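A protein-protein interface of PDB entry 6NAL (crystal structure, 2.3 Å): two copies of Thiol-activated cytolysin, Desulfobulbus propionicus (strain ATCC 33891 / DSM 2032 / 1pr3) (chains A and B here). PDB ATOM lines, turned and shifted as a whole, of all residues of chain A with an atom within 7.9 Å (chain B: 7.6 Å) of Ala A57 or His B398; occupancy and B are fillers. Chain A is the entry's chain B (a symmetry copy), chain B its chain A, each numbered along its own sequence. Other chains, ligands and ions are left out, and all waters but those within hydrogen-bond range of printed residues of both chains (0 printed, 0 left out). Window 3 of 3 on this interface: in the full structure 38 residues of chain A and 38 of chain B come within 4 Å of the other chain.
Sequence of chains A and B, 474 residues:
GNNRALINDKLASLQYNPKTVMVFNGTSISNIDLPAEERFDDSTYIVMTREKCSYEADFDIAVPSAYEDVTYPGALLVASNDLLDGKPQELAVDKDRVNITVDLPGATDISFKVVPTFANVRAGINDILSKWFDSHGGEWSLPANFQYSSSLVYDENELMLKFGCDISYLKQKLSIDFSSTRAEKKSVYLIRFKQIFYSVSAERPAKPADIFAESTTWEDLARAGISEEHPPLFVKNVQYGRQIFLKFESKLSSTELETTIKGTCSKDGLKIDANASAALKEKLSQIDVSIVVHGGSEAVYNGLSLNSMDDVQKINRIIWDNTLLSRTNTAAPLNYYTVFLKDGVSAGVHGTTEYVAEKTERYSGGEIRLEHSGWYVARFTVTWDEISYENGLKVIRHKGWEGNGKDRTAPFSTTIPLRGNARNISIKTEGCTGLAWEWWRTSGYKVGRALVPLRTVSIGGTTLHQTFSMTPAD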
ATOM      1  N   PHE A  24     -15.698 -28.006   8.135  1.00  0.00           N
ATOM      2  CA  PHE A  24     -14.805 -27.292   7.249  1.00  0.00           C
ATOM      3  C   PHE A  24     -13.666 -26.683   8.054  1.00  0.00           C
ATOM      4  O   PHE A  24     -13.883 -25.993   9.054  1.00  0.00           O
ATOM      5  CB  PHE A  24     -15.549 -26.208   6.476  1.00  0.00           C
ATOM      6  CG  PHE A  24     -14.708 -25.585   5.412  1.00  0.00           C
ATOM      7  CD1 PHE A  24     -14.532 -26.214   4.190  1.00  0.00           C
ATOM      8  CD2 PHE A  24     -14.053 -24.387   5.650  1.00  0.00           C
ATOM      9  CE1 PHE A  24     -13.718 -25.648   3.195  1.00  0.00           C
ATOM     10  CE2 PHE A  24     -13.248 -23.800   4.664  1.00  0.00           C
ATOM     11  CZ  PHE A  24     -13.069 -24.434   3.443  1.00  0.00           C
ATOM     12  N   SER A  54     -13.147 -12.433   7.650  1.00  0.00           N
ATOM     13  CA  SER A  54     -13.564 -13.807   7.403  1.00  0.00           C
ATOM     14  C   SER A  54     -14.816 -13.847   6.536  1.00  0.00           C
ATOM     15  O   SER A  54     -15.665 -12.971   6.607  1.00  0.00           O
ATOM     16  CB  SER A  54     -13.828 -14.587   8.688  1.00  0.00           C
ATOM     17  OG  SER A  54     -15.081 -14.250   9.215  1.00  0.00           O
ATOM     18  N   TYR A  55     -14.917 -14.895   5.728  1.00  0.00           N
ATOM     19  CA  TYR A  55     -16.042 -15.137   4.842  1.00  0.00           C
ATOM     20  C   TYR A  55     -16.723 -16.428   5.222  1.00  0.00           C
ATOM     21  O   TYR A  55     -16.063 -17.468   5.333  1.00  0.00           O
ATOM     22  CB  TYR A  55     -15.554 -15.238   3.425  1.00  0.00           C
ATOM     23  CG  TYR A  55     -16.631 -15.435   2.404  1.00  0.00           C
ATOM     24  CD1 TYR A  55     -17.418 -14.373   2.013  1.00  0.00           C
ATOM     25  CD2 TYR A  55     -16.853 -16.696   1.805  1.00  0.00           C
ATOM     26  CE1 TYR A  55     -18.395 -14.526   1.069  1.00  0.00           C
ATOM     27  CE2 TYR A  55     -17.822 -16.855   0.852  1.00  0.00           C
ATOM     28  CZ  TYR A  55     -18.585 -15.774   0.492  1.00  0.00           C
ATOM     29  OH  TYR A  55     -19.555 -15.913  -0.435  1.00  0.00           O
ATOM     30  N   GLU A  56     -18.033 -16.359   5.384  1.00  0.00           N
ATOM     31  CA  GLU A  56     -18.844 -17.516   5.707  1.00  0.00           C
ATOM     32  C   GLU A  56     -19.856 -17.732   4.606  1.00  0.00           C
ATOM     33  O   GLU A  56     -20.571 -16.795   4.237  1.00  0.00           O
ATOM     34  CB  GLU A  56     -19.618 -17.333   6.994  1.00  0.00           C
ATOM     35  CG  GLU A  56     -18.816 -16.789   8.100  1.00  0.00           C
ATOM     36  CD  GLU A  56     -19.562 -16.895   9.407  1.00  0.00           C
ATOM     37  OE1 GLU A  56     -20.698 -17.485   9.398  1.00  0.00           O
ATOM     38  OE2 GLU A  56     -19.001 -16.392  10.415  1.00  0.00           O
ATOM     39  N   ALA A  57     -19.989 -18.981   4.173  1.00  0.00           N
ATOM     40  CA  ALA A  57     -21.003 -19.348   3.191  1.00  0.00           C
ATOM     41  C   ALA A  57     -21.154 -20.862   3.161  1.00  0.00           C
ATOM     42  O   ALA A  57     -20.334 -21.599   3.703  1.00  0.00           O
ATOM     43  CB  ALA A  57     -20.617 -18.871   1.784  1.00  0.00           C
ATOM     44  N   ASP A  58     -22.162 -21.318   2.431  1.00  0.00           N
ATOM     45  CA  ASP A  58     -22.319 -22.745   2.189  1.00  0.00           C
ATOM     46  C   ASP A  58     -21.217 -23.249   1.264  1.00  0.00           C
ATOM     47  O   ASP A  58     -20.804 -22.575   0.318  1.00  0.00           O
ATOM     48  CB  ASP A  58     -23.697 -23.049   1.595  1.00  0.00           C
ATOM     49  CG  ASP A  58     -24.846 -22.745   2.567  1.00  0.00           C
ATOM     50  OD1 ASP A  58     -24.725 -22.980   3.817  1.00  0.00           O
ATOM     51  OD2 ASP A  58     -25.887 -22.270   2.060  1.00  0.00           O
ATOM     52  N   PHE A  59     -20.752 -24.447   1.542  1.00  0.00           N
ATOM     53  CA  PHE A  59     -19.621 -25.032   0.854  1.00  0.00           C
ATOM     54  C   PHE A  59     -20.206 -26.036  -0.129  1.00  0.00           C
ATOM     55  O   PHE A  59     -20.649 -27.121   0.256  1.00  0.00           O
ATOM     56  CB  PHE A  59     -18.679 -25.646   1.880  1.00  0.00           C
ATOM     57  CG  PHE A  59     -17.408 -26.203   1.314  1.00  0.00           C
ATOM     58  CD1 PHE A  59     -16.652 -25.495   0.418  1.00  0.00           C
ATOM     59  CD2 PHE A  59     -16.963 -27.441   1.704  1.00  0.00           C
ATOM     60  CE1 PHE A  59     -15.490 -26.029  -0.096  1.00  0.00           C
ATOM     61  CE2 PHE A  59     -15.805 -27.962   1.211  1.00  0.00           C
ATOM     62  CZ  PHE A  59     -15.080 -27.282   0.301  1.00  0.00           C
ATOM     63  N   ASP A  60     -20.210 -25.644  -1.404  1.00  0.00           N
ATOM     64  CA  ASP A  60     -20.529 -26.541  -2.494  1.00  0.00           C
ATOM     65  C   ASP A  60     -19.350 -27.490  -2.716  1.00  0.00           C
ATOM     66  O   ASP A  60     -18.243 -27.029  -2.998  1.00  0.00           O
ATOM     67  CB  ASP A  60     -20.822 -25.763  -3.783  1.00  0.00           C
ATOM     68  CG  ASP A  60     -22.312 -25.439  -3.972  1.00  0.00           C
ATOM     69  OD1 ASP A  60     -23.157 -25.751  -3.079  1.00  0.00           O
ATOM     70  OD2 ASP A  60     -22.630 -24.830  -5.019  1.00  0.00           O
ATOM     71  N   GLN A 147     -23.930 -19.577 -13.964  1.00  0.00           N
ATOM     72  CA  GLN A 147     -23.501 -18.817 -12.813  1.00  0.00           C
ATOM     73  C   GLN A 147     -22.174 -18.130 -13.136  1.00  0.00           C
ATOM     74  O   GLN A 147     -21.342 -18.660 -13.881  1.00  0.00           O
ATOM     75  CB  GLN A 147     -23.388 -19.661 -11.545  1.00  0.00           C
ATOM     76  CG  GLN A 147     -23.202 -18.644 -10.340  1.00  0.00           C
ATOM     77  CD  GLN A 147     -23.068 -19.330  -9.021  1.00  0.00           C
ATOM     78  OE1 GLN A 147     -23.655 -18.859  -8.037  1.00  0.00           O
ATOM     79  NE2 GLN A 147     -22.300 -20.442  -8.969  1.00  0.00           N
ATOM     80  N   LEU A 161     -13.970 -21.913  -0.880  1.00  0.00           N
ATOM     81  CA  LEU A 161     -15.252 -21.523  -0.297  1.00  0.00           C
ATOM     82  C   LEU A 161     -16.063 -20.582  -1.192  1.00  0.00           C
ATOM     83  O   LEU A 161     -17.294 -20.692  -1.255  1.00  0.00           O
ATOM     84  CB  LEU A 161     -14.999 -20.870   1.053  1.00  0.00           C
ATOM     85  CG  LEU A 161     -16.159 -20.763   2.023  1.00  0.00           C
ATOM     86  CD1 LEU A 161     -16.953 -22.020   2.130  1.00  0.00           C
ATOM     87  CD2 LEU A 161     -15.633 -20.393   3.389  1.00  0.00           C
ATOM     88  N   LYS A 162     -15.430 -19.616  -1.845  1.00  0.00           N
ATOM     89  CA  LYS A 162     -16.214 -18.707  -2.687  1.00  0.00           C
ATOM     90  C   LYS A 162     -16.684 -19.401  -3.955  1.00  0.00           C
ATOM     91  O   LYS A 162     -17.806 -19.189  -4.393  1.00  0.00           O
ATOM     92  CB  LYS A 162     -15.401 -17.450  -3.006  1.00  0.00           C
ATOM     93  CG  LYS A 162     -15.312 -16.531  -1.774  1.00  0.00           C
ATOM     94  CD  LYS A 162     -14.533 -15.225  -1.966  1.00  0.00           C
ATOM     95  CE  LYS A 162     -14.748 -14.324  -0.732  1.00  0.00           C
ATOM     96  NZ  LYS A 162     -14.220 -12.946  -0.804  1.00  0.00           N
ATOM     97  N   VAL A 349     -22.346 -28.779   4.400  1.00  0.00           N
ATOM     98  CA  VAL A 349     -21.678 -28.033   5.461  1.00  0.00           C
ATOM     99  C   VAL A 349     -21.562 -26.552   5.118  1.00  0.00           C
ATOM    100  O   VAL A 349     -21.397 -26.175   3.954  1.00  0.00           O
ATOM    101  CB  VAL A 349     -20.282 -28.625   5.736  1.00  0.00           C
ATOM    102  CG1 VAL A 349     -20.412 -30.084   6.293  1.00  0.00           C
ATOM    103  CG2 VAL A 349     -19.464 -28.660   4.461  1.00  0.00           C
ATOM    104  N   HIS A 350     -21.661 -25.729   6.163  1.00  0.00           N
ATOM    105  CA  HIS A 350     -21.305 -24.319   6.192  1.00  0.00           C
ATOM    106  C   HIS A 350     -19.805 -24.183   6.435  1.00  0.00           C
ATOM    107  O   HIS A 350     -19.188 -24.988   7.126  1.00  0.00           O
ATOM    108  CB  HIS A 350     -22.102 -23.618   7.312  1.00  0.00           C
ATOM    109  CG  HIS A 350     -22.257 -22.134   7.132  1.00  0.00           C
ATOM    110  ND1 HIS A 350     -23.112 -21.581   6.196  1.00  0.00           N
ATOM    111  CD2 HIS A 350     -21.670 -21.085   7.771  1.00  0.00           C
ATOM    112  CE1 HIS A 350     -23.031 -20.260   6.256  1.00  0.00           C
ATOM    113  NE2 HIS A 350     -22.163 -19.933   7.200  1.00  0.00           N
ATOM    114  N   GLY A 351     -19.211 -23.161   5.849  1.00  0.00           N
ATOM    115  CA  GLY A 351     -17.785 -22.967   5.948  1.00  0.00           C
ATOM    116  C   GLY A 351     -17.476 -21.538   6.327  1.00  0.00           C
ATOM    117  O   GLY A 351     -18.287 -20.638   6.118  1.00  0.00           O
ATOM    118  N   THR A 352     -16.321 -21.372   7.003  1.00  0.00           N
ATOM    119  CA  THR A 352     -15.758 -20.091   7.409  1.00  0.00           C
ATOM    120  C   THR A 352     -14.264 -20.103   7.164  1.00  0.00           C
ATOM    121  O   THR A 352     -13.584 -21.095   7.453  1.00  0.00           O
ATOM    122  CB  THR A 352     -15.974 -19.764   8.884  1.00  0.00           C
ATOM    123  OG1 THR A 352     -17.373 -19.675   9.152  1.00  0.00           O
ATOM    124  CG2 THR A 352     -15.318 -18.418   9.224  1.00  0.00           C
ATOM    125  N   THR A 353     -13.739 -18.984   6.687  1.00  0.00           N
ATOM    126  CA  THR A 353     -12.290 -18.871   6.541  1.00  0.00           C
ATOM    127  C   THR A 353     -11.873 -17.432   6.750  1.00  0.00           C
ATOM    128  O   THR A 353     -12.620 -16.511   6.422  1.00  0.00           O
ATOM    129  CB  THR A 353     -11.851 -19.360   5.172  1.00  0.00           C
ATOM    130  OG1 THR A 353     -10.448 -19.598   5.180  1.00  0.00           O
ATOM    131  CG2 THR A 353     -12.188 -18.329   4.092  1.00  0.00           C
ATOM    132  N   VAL B 382     -32.095 -13.830  -5.652  1.00  0.00           N
ATOM    133  CA  VAL B 382     -31.503 -12.644  -5.052  1.00  0.00           C
ATOM    134  C   VAL B 382     -30.553 -13.074  -3.942  1.00  0.00           C
ATOM    135  O   VAL B 382     -30.925 -13.869  -3.079  1.00  0.00           O
ATOM    136  CB  VAL B 382     -32.564 -11.683  -4.514  1.00  0.00           C
ATOM    137  CG1 VAL B 382     -31.850 -10.472  -3.917  1.00  0.00           C
ATOM    138  CG2 VAL B 382     -33.499 -11.277  -5.610  1.00  0.00           C
ATOM    139  N   THR B 383     -29.309 -12.591  -4.000  1.00  0.00           N
ATOM    140  CA  THR B 383     -28.281 -12.907  -3.022  1.00  0.00           C
ATOM    141  C   THR B 383     -27.557 -11.622  -2.617  1.00  0.00           C
ATOM    142  O   THR B 383     -27.605 -10.607  -3.314  1.00  0.00           O
ATOM    143  CB  THR B 383     -27.280 -13.946  -3.570  1.00  0.00           C
ATOM    144  OG1 THR B 383     -26.499 -13.332  -4.596  1.00  0.00           O
ATOM    145  CG2 THR B 383     -28.026 -15.217  -4.115  1.00  0.00           C
ATOM    146  N   TRP B 384     -26.907 -11.657  -1.465  1.00  0.00           N
ATOM    147  CA  TRP B 384     -26.159 -10.494  -1.006  1.00  0.00           C
ATOM    148  C   TRP B 384     -25.221 -10.924   0.103  1.00  0.00           C
ATOM    149  O   TRP B 384     -25.287 -12.045   0.611  1.00  0.00           O
ATOM    150  CB  TRP B 384     -27.065  -9.363  -0.507  1.00  0.00           C
ATOM    151  CG  TRP B 384     -27.939  -9.734   0.641  1.00  0.00           C
ATOM    152  CD1 TRP B 384     -27.634  -9.636   1.951  1.00  0.00           C
ATOM    153  CD2 TRP B 384     -29.273 -10.262   0.575  1.00  0.00           C
ATOM    154  NE1 TRP B 384     -28.675 -10.123   2.723  1.00  0.00           N
ATOM    155  CE2 TRP B 384     -29.699 -10.498   1.899  1.00  0.00           C
ATOM    156  CE3 TRP B 384     -30.148 -10.557  -0.472  1.00  0.00           C
ATOM    157  CZ2 TRP B 384     -30.958 -11.018   2.201  1.00  0.00           C
ATOM    158  CZ3 TRP B 384     -31.403 -11.076  -0.171  1.00  0.00           C
ATOM    159  CH2 TRP B 384     -31.799 -11.284   1.156  1.00  0.00           C
ATOM    160  N   ASP B 385     -24.365  -9.992   0.498  1.00  0.00           N
ATOM    161  CA  ASP B 385     -23.422 -10.220   1.577  1.00  0.00           C
ATOM    162  C   ASP B 385     -23.812  -9.354   2.760  1.00  0.00           C
ATOM    163  O   ASP B 385     -24.230  -8.216   2.581  1.00  0.00           O
ATOM    164  CB  ASP B 385     -21.997  -9.889   1.132  1.00  0.00           C
ATOM    165  CG  ASP B 385     -21.343 -11.008   0.316  1.00  0.00           C
ATOM    166  OD1 ASP B 385     -21.762 -12.206   0.448  1.00  0.00           O
ATOM    167  OD2 ASP B 385     -20.383 -10.668  -0.438  1.00  0.00           O
ATOM    168  N   GLU B 386     -23.678  -9.886   3.967  1.00  0.00           N
ATOM    169  CA  GLU B 386     -23.925  -9.108   5.169  1.00  0.00           C
ATOM    170  C   GLU B 386     -22.640  -8.928   5.971  1.00  0.00           C
ATOM    171  O   GLU B 386     -21.930  -9.904   6.268  1.00  0.00           O
ATOM    172  CB  GLU B 386     -25.008  -9.765   6.022  1.00  0.00           C
ATOM    173  CG  GLU B 386     -26.421  -9.523   5.498  1.00  0.00           C
ATOM    174  CD  GLU B 386     -27.499 -10.358   6.207  1.00  0.00           C
ATOM    175  OE1 GLU B 386     -27.222 -10.896   7.315  1.00  0.00           O
ATOM    176  OE2 GLU B 386     -28.632 -10.459   5.650  1.00  0.00           O
ATOM    177  N   VAL B 395     -16.529  -9.652   9.475  1.00  0.00           N
ATOM    178  CA  VAL B 395     -17.151 -10.919   9.089  1.00  0.00           C
ATOM    179  C   VAL B 395     -18.106 -10.658   7.938  1.00  0.00           C
ATOM    180  O   VAL B 395     -18.921  -9.728   7.997  1.00  0.00           O
ATOM    181  CB  VAL B 395     -17.899 -11.566  10.272  1.00  0.00           C
ATOM    182  CG1 VAL B 395     -18.583 -12.856   9.905  1.00  0.00           C
ATOM    183  CG2 VAL B 395     -16.956 -11.867  11.392  1.00  0.00           C
ATOM    184  N   ILE B 396     -18.001 -11.470   6.898  1.00  0.00           N
ATOM    185  CA  ILE B 396     -18.786 -11.329   5.681  1.00  0.00           C
ATOM    186  C   ILE B 396     -19.550 -12.627   5.495  1.00  0.00           C
ATOM    187  O   ILE B 396     -18.932 -13.679   5.317  1.00  0.00           O
ATOM    188  CB  ILE B 396     -17.895 -11.035   4.468  1.00  0.00           C
ATOM    189  CG1 ILE B 396     -17.173  -9.693   4.677  1.00  0.00           C
ATOM    190  CG2 ILE B 396     -18.716 -10.955   3.200  1.00  0.00           C
ATOM    191  CD1 ILE B 396     -16.021  -9.465   3.704  1.00  0.00           C
ATOM    192  N   ARG B 397     -20.883 -12.564   5.573  1.00  0.00           N
ATOM    193  CA  ARG B 397     -21.724 -13.746   5.421  1.00  0.00           C
ATOM    194  C   ARG B 397     -22.555 -13.666   4.140  1.00  0.00           C
ATOM    195  O   ARG B 397     -23.336 -12.728   3.960  1.00  0.00           O
ATOM    196  CB  ARG B 397     -22.657 -13.928   6.616  1.00  0.00           C
ATOM    197  CG  ARG B 397     -21.964 -14.023   7.940  1.00  0.00           C
ATOM    198  CD  ARG B 397     -22.972 -14.229   9.107  1.00  0.00           C
ATOM    199  NE  ARG B 397     -22.243 -14.608  10.312  1.00  0.00           N
ATOM    200  CZ  ARG B 397     -21.871 -13.751  11.260  1.00  0.00           C
ATOM    201  NH1 ARG B 397     -22.181 -12.480  11.157  1.00  0.00           N
ATOM    202  NH2 ARG B 397     -21.187 -14.169  12.312  1.00  0.00           N
ATOM    203  N   HIS B 398     -22.364 -14.638   3.248  1.00  0.00           N
ATOM    204  CA  HIS B 398     -23.189 -14.767   2.061  1.00  0.00           C
ATOM    205  C   HIS B 398     -24.596 -15.189   2.446  1.00  0.00           C
ATOM    206  O   HIS B 398     -24.777 -16.098   3.245  1.00  0.00           O
ATOM    207  CB  HIS B 398     -22.572 -15.786   1.107  1.00  0.00           C
ATOM    208  CG  HIS B 398     -23.266 -15.864  -0.217  1.00  0.00           C
ATOM    209  ND1 HIS B 398     -23.445 -14.772  -1.037  1.00  0.00           N
ATOM    210  CD2 HIS B 398     -23.820 -16.909  -0.861  1.00  0.00           C
ATOM    211  CE1 HIS B 398     -24.092 -15.145  -2.123  1.00  0.00           C
ATOM    212  NE2 HIS B 398     -24.339 -16.438  -2.035  1.00  0.00           N
ATOM    213  N   LYS B 399     -25.596 -14.512   1.891  1.00  0.00           N
ATOM    214  CA  LYS B 399     -26.987 -14.757   2.233  1.00  0.00           C
ATOM    215  C   LYS B 399     -27.847 -14.765   0.967  1.00  0.00           C
ATOM    216  O   LYS B 399     -27.430 -14.337  -0.108  1.00  0.00           O
ATOM    217  CB  LYS B 399     -27.536 -13.707   3.191  1.00  0.00           C
ATOM    218  CG  LYS B 399     -26.806 -13.554   4.494  1.00  0.00           C
ATOM    219  CD  LYS B 399     -27.230 -14.594   5.505  1.00  0.00           C
ATOM    220  CE  LYS B 399     -26.833 -14.123   6.907  1.00  0.00           C
ATOM    221  NZ  LYS B 399     -26.591 -15.252   7.851  1.00  0.00           N
ATOM    222  N   GLY B 400     -29.062 -15.266   1.118  1.00  0.00           N
ATOM    223  CA  GLY B 400     -29.939 -15.484  -0.003  1.00  0.00           C
ATOM    224  C   GLY B 400     -31.372 -15.256   0.403  1.00  0.00           C
ATOM    225  O   GLY B 400     -31.802 -15.638   1.491  1.00  0.00           O
ATOM    226  N   ASN B 404     -35.627 -17.756  -3.425  1.00  0.00           N
ATOM    227  CA  ASN B 404     -34.796 -17.978  -4.591  1.00  0.00           C
ATOM    228  C   ASN B 404     -35.183 -19.270  -5.274  1.00  0.00           C
ATOM    229  O   ASN B 404     -35.499 -20.259  -4.616  1.00  0.00           O
ATOM    230  CB  ASN B 404     -33.330 -18.021  -4.182  1.00  0.00           C
ATOM    231  CG  ASN B 404     -32.780 -16.639  -3.936  1.00  0.00           C
ATOM    232  OD1 ASN B 404     -33.489 -15.634  -4.099  1.00  0.00           O
ATOM    233  ND2 ASN B 404     -31.550 -16.570  -3.515  1.00  0.00           N
ATOM    234  N   ARG B 423     -24.344  -5.692   1.399  1.00  0.00           N
ATOM    235  CA  ARG B 423     -23.601  -5.233   0.234  1.00  0.00           C
ATOM    236  C   ARG B 423     -23.732  -6.238  -0.900  1.00  0.00           C
ATOM    237  O   ARG B 423     -24.175  -7.385  -0.709  1.00  0.00           O
ATOM    238  CB  ARG B 423     -22.096  -5.102   0.487  1.00  0.00           C
ATOM    239  CG  ARG B 423     -21.684  -4.562   1.807  1.00  0.00           C
ATOM    240  CD  ARG B 423     -21.488  -3.037   1.732  1.00  0.00           C
ATOM    241  NE  ARG B 423     -20.776  -2.579   2.927  1.00  0.00           N
ATOM    242  CZ  ARG B 423     -21.370  -2.068   3.992  1.00  0.00           C
ATOM    243  NH1 ARG B 423     -22.682  -1.915   3.965  1.00  0.00           N
ATOM    244  NH2 ARG B 423     -20.653  -1.703   5.062  1.00  0.00           N
ATOM    245  N   ASN B 424     -23.251  -5.833  -2.084  1.00  0.00           N
ATOM    246  CA  ASN B 424     -22.914  -6.794  -3.154  1.00  0.00           C
ATOM    247  C   ASN B 424     -24.132  -7.576  -3.644  1.00  0.00           C
ATOM    248  O   ASN B 424     -24.124  -8.804  -3.767  1.00  0.00           O
ATOM    249  CB  ASN B 424     -21.810  -7.723  -2.653  1.00  0.00           C
ATOM    250  CG  ASN B 424     -21.046  -8.369  -3.765  1.00  0.00           C
ATOM    251  OD1 ASN B 424     -21.317  -8.123  -4.936  1.00  0.00           O
ATOM    252  ND2 ASN B 424     -20.092  -9.233  -3.409  1.00  0.00           N
ATOM    253  N   SER B 426     -26.894  -9.215  -5.813  1.00  0.00           N
ATOM    254  CA  SER B 426     -27.006  -9.856  -7.112  1.00  0.00           C
ATOM    255  C   SER B 426     -28.449 -10.282  -7.334  1.00  0.00           C
ATOM    256  O   SER B 426     -29.110 -10.785  -6.416  1.00  0.00           O
ATOM    257  CB  SER B 426     -26.045 -11.030  -7.202  1.00  0.00           C
ATOM    258  OG  SER B 426     -26.505 -12.041  -8.081  1.00  0.00           O
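O of Ser A54 lies within hydrogen-bond range of N of Ile B396, at 2.8 Å. The backbone carbonyl oxygen of Ile B396 sits at hydrogen-bond distance from the backbone NH of Glu A56. NE of Arg B397 lies within salt-bridge range of OE1 of Glu A56, 3.4 Å away. The backbone NH of His B398 sits at hydrogen-bond distance from the backbone carbonyl oxygen of Glu A56, 3.0 Å away.
The side-chain carboxylate (OD1) of Asp B385 lies close to a ring nitrogen (ND1) of His B398 (3.4 Å). The backbone carbonyl oxygen of Arg B397 is in hydrogen-bond range of the backbone NH of Glu B386 (2.9 Å). The backbone NH of Tyr A55 sits at hydrogen-bond distance from the backbone carbonyl oxygen of Thr A353. N of Gly A351 lies within hydrogen-bond range of O of Ala A57, 2.9 Å away.
O of Ser A54 touches CA of Val B395 (3.5 Å). Tyr A55 touches Ile B396. OH of Tyr A55 touches CB of His B398, at 3.4 Å. Val B395 touches Glu A56 (CG1 to OE2, 3.6 Å). His B398 touches Ala A57 (CB to CB, 3.7 Å).
Of chain B, only His B398 (3.7 Å) comes within 4 Å of Ala A57. His B398 touches just these residues of chain A: Tyr A55, Glu A56 and Ala A57. Of the printed residues of chain B, Glu A56 touches Val B395, Ile B396, Arg B397 and His B398. Of the printed residues of chain A, Val B395 touches Ser A54 and Glu A56. Printed residues of chain A within 4 Å of Arg B397: Glu A56. Of the printed residues of chain B, Tyr A55 touches Ile B396 and His B398. Of the printed residues of chain B, Ser A54 touches Val B395 and Ile B396. Glu B386 touches none of the printed residues of chain A. The nearest residue of chain B that does not touch Ala A57 is Ile B396 (5.5 Å). The nearest printed residue of chain B that does not touch Glu A56 is Lys B399 (6.0 Å).
Of the 15 printed residues of chain B, 4 touch a printed residue of chain A. Hydrophobic or aromatic side chains of chain B that line the printed part of chain A: Val B395, Ile B396 and His B398. Hydrophobic or aromatic side chains of chain A that line the printed part of chain B: Tyr A55 and Ala A57. Among the printed residues, 9 pairs touch across the chains. Among the printed residues, Asp or Glu carboxylates within 4 Å of a Lys or Arg side-chain nitrogen of the other chain: Glu A56 with Arg B397 (3.4 Å).
No position is printed for both chains.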
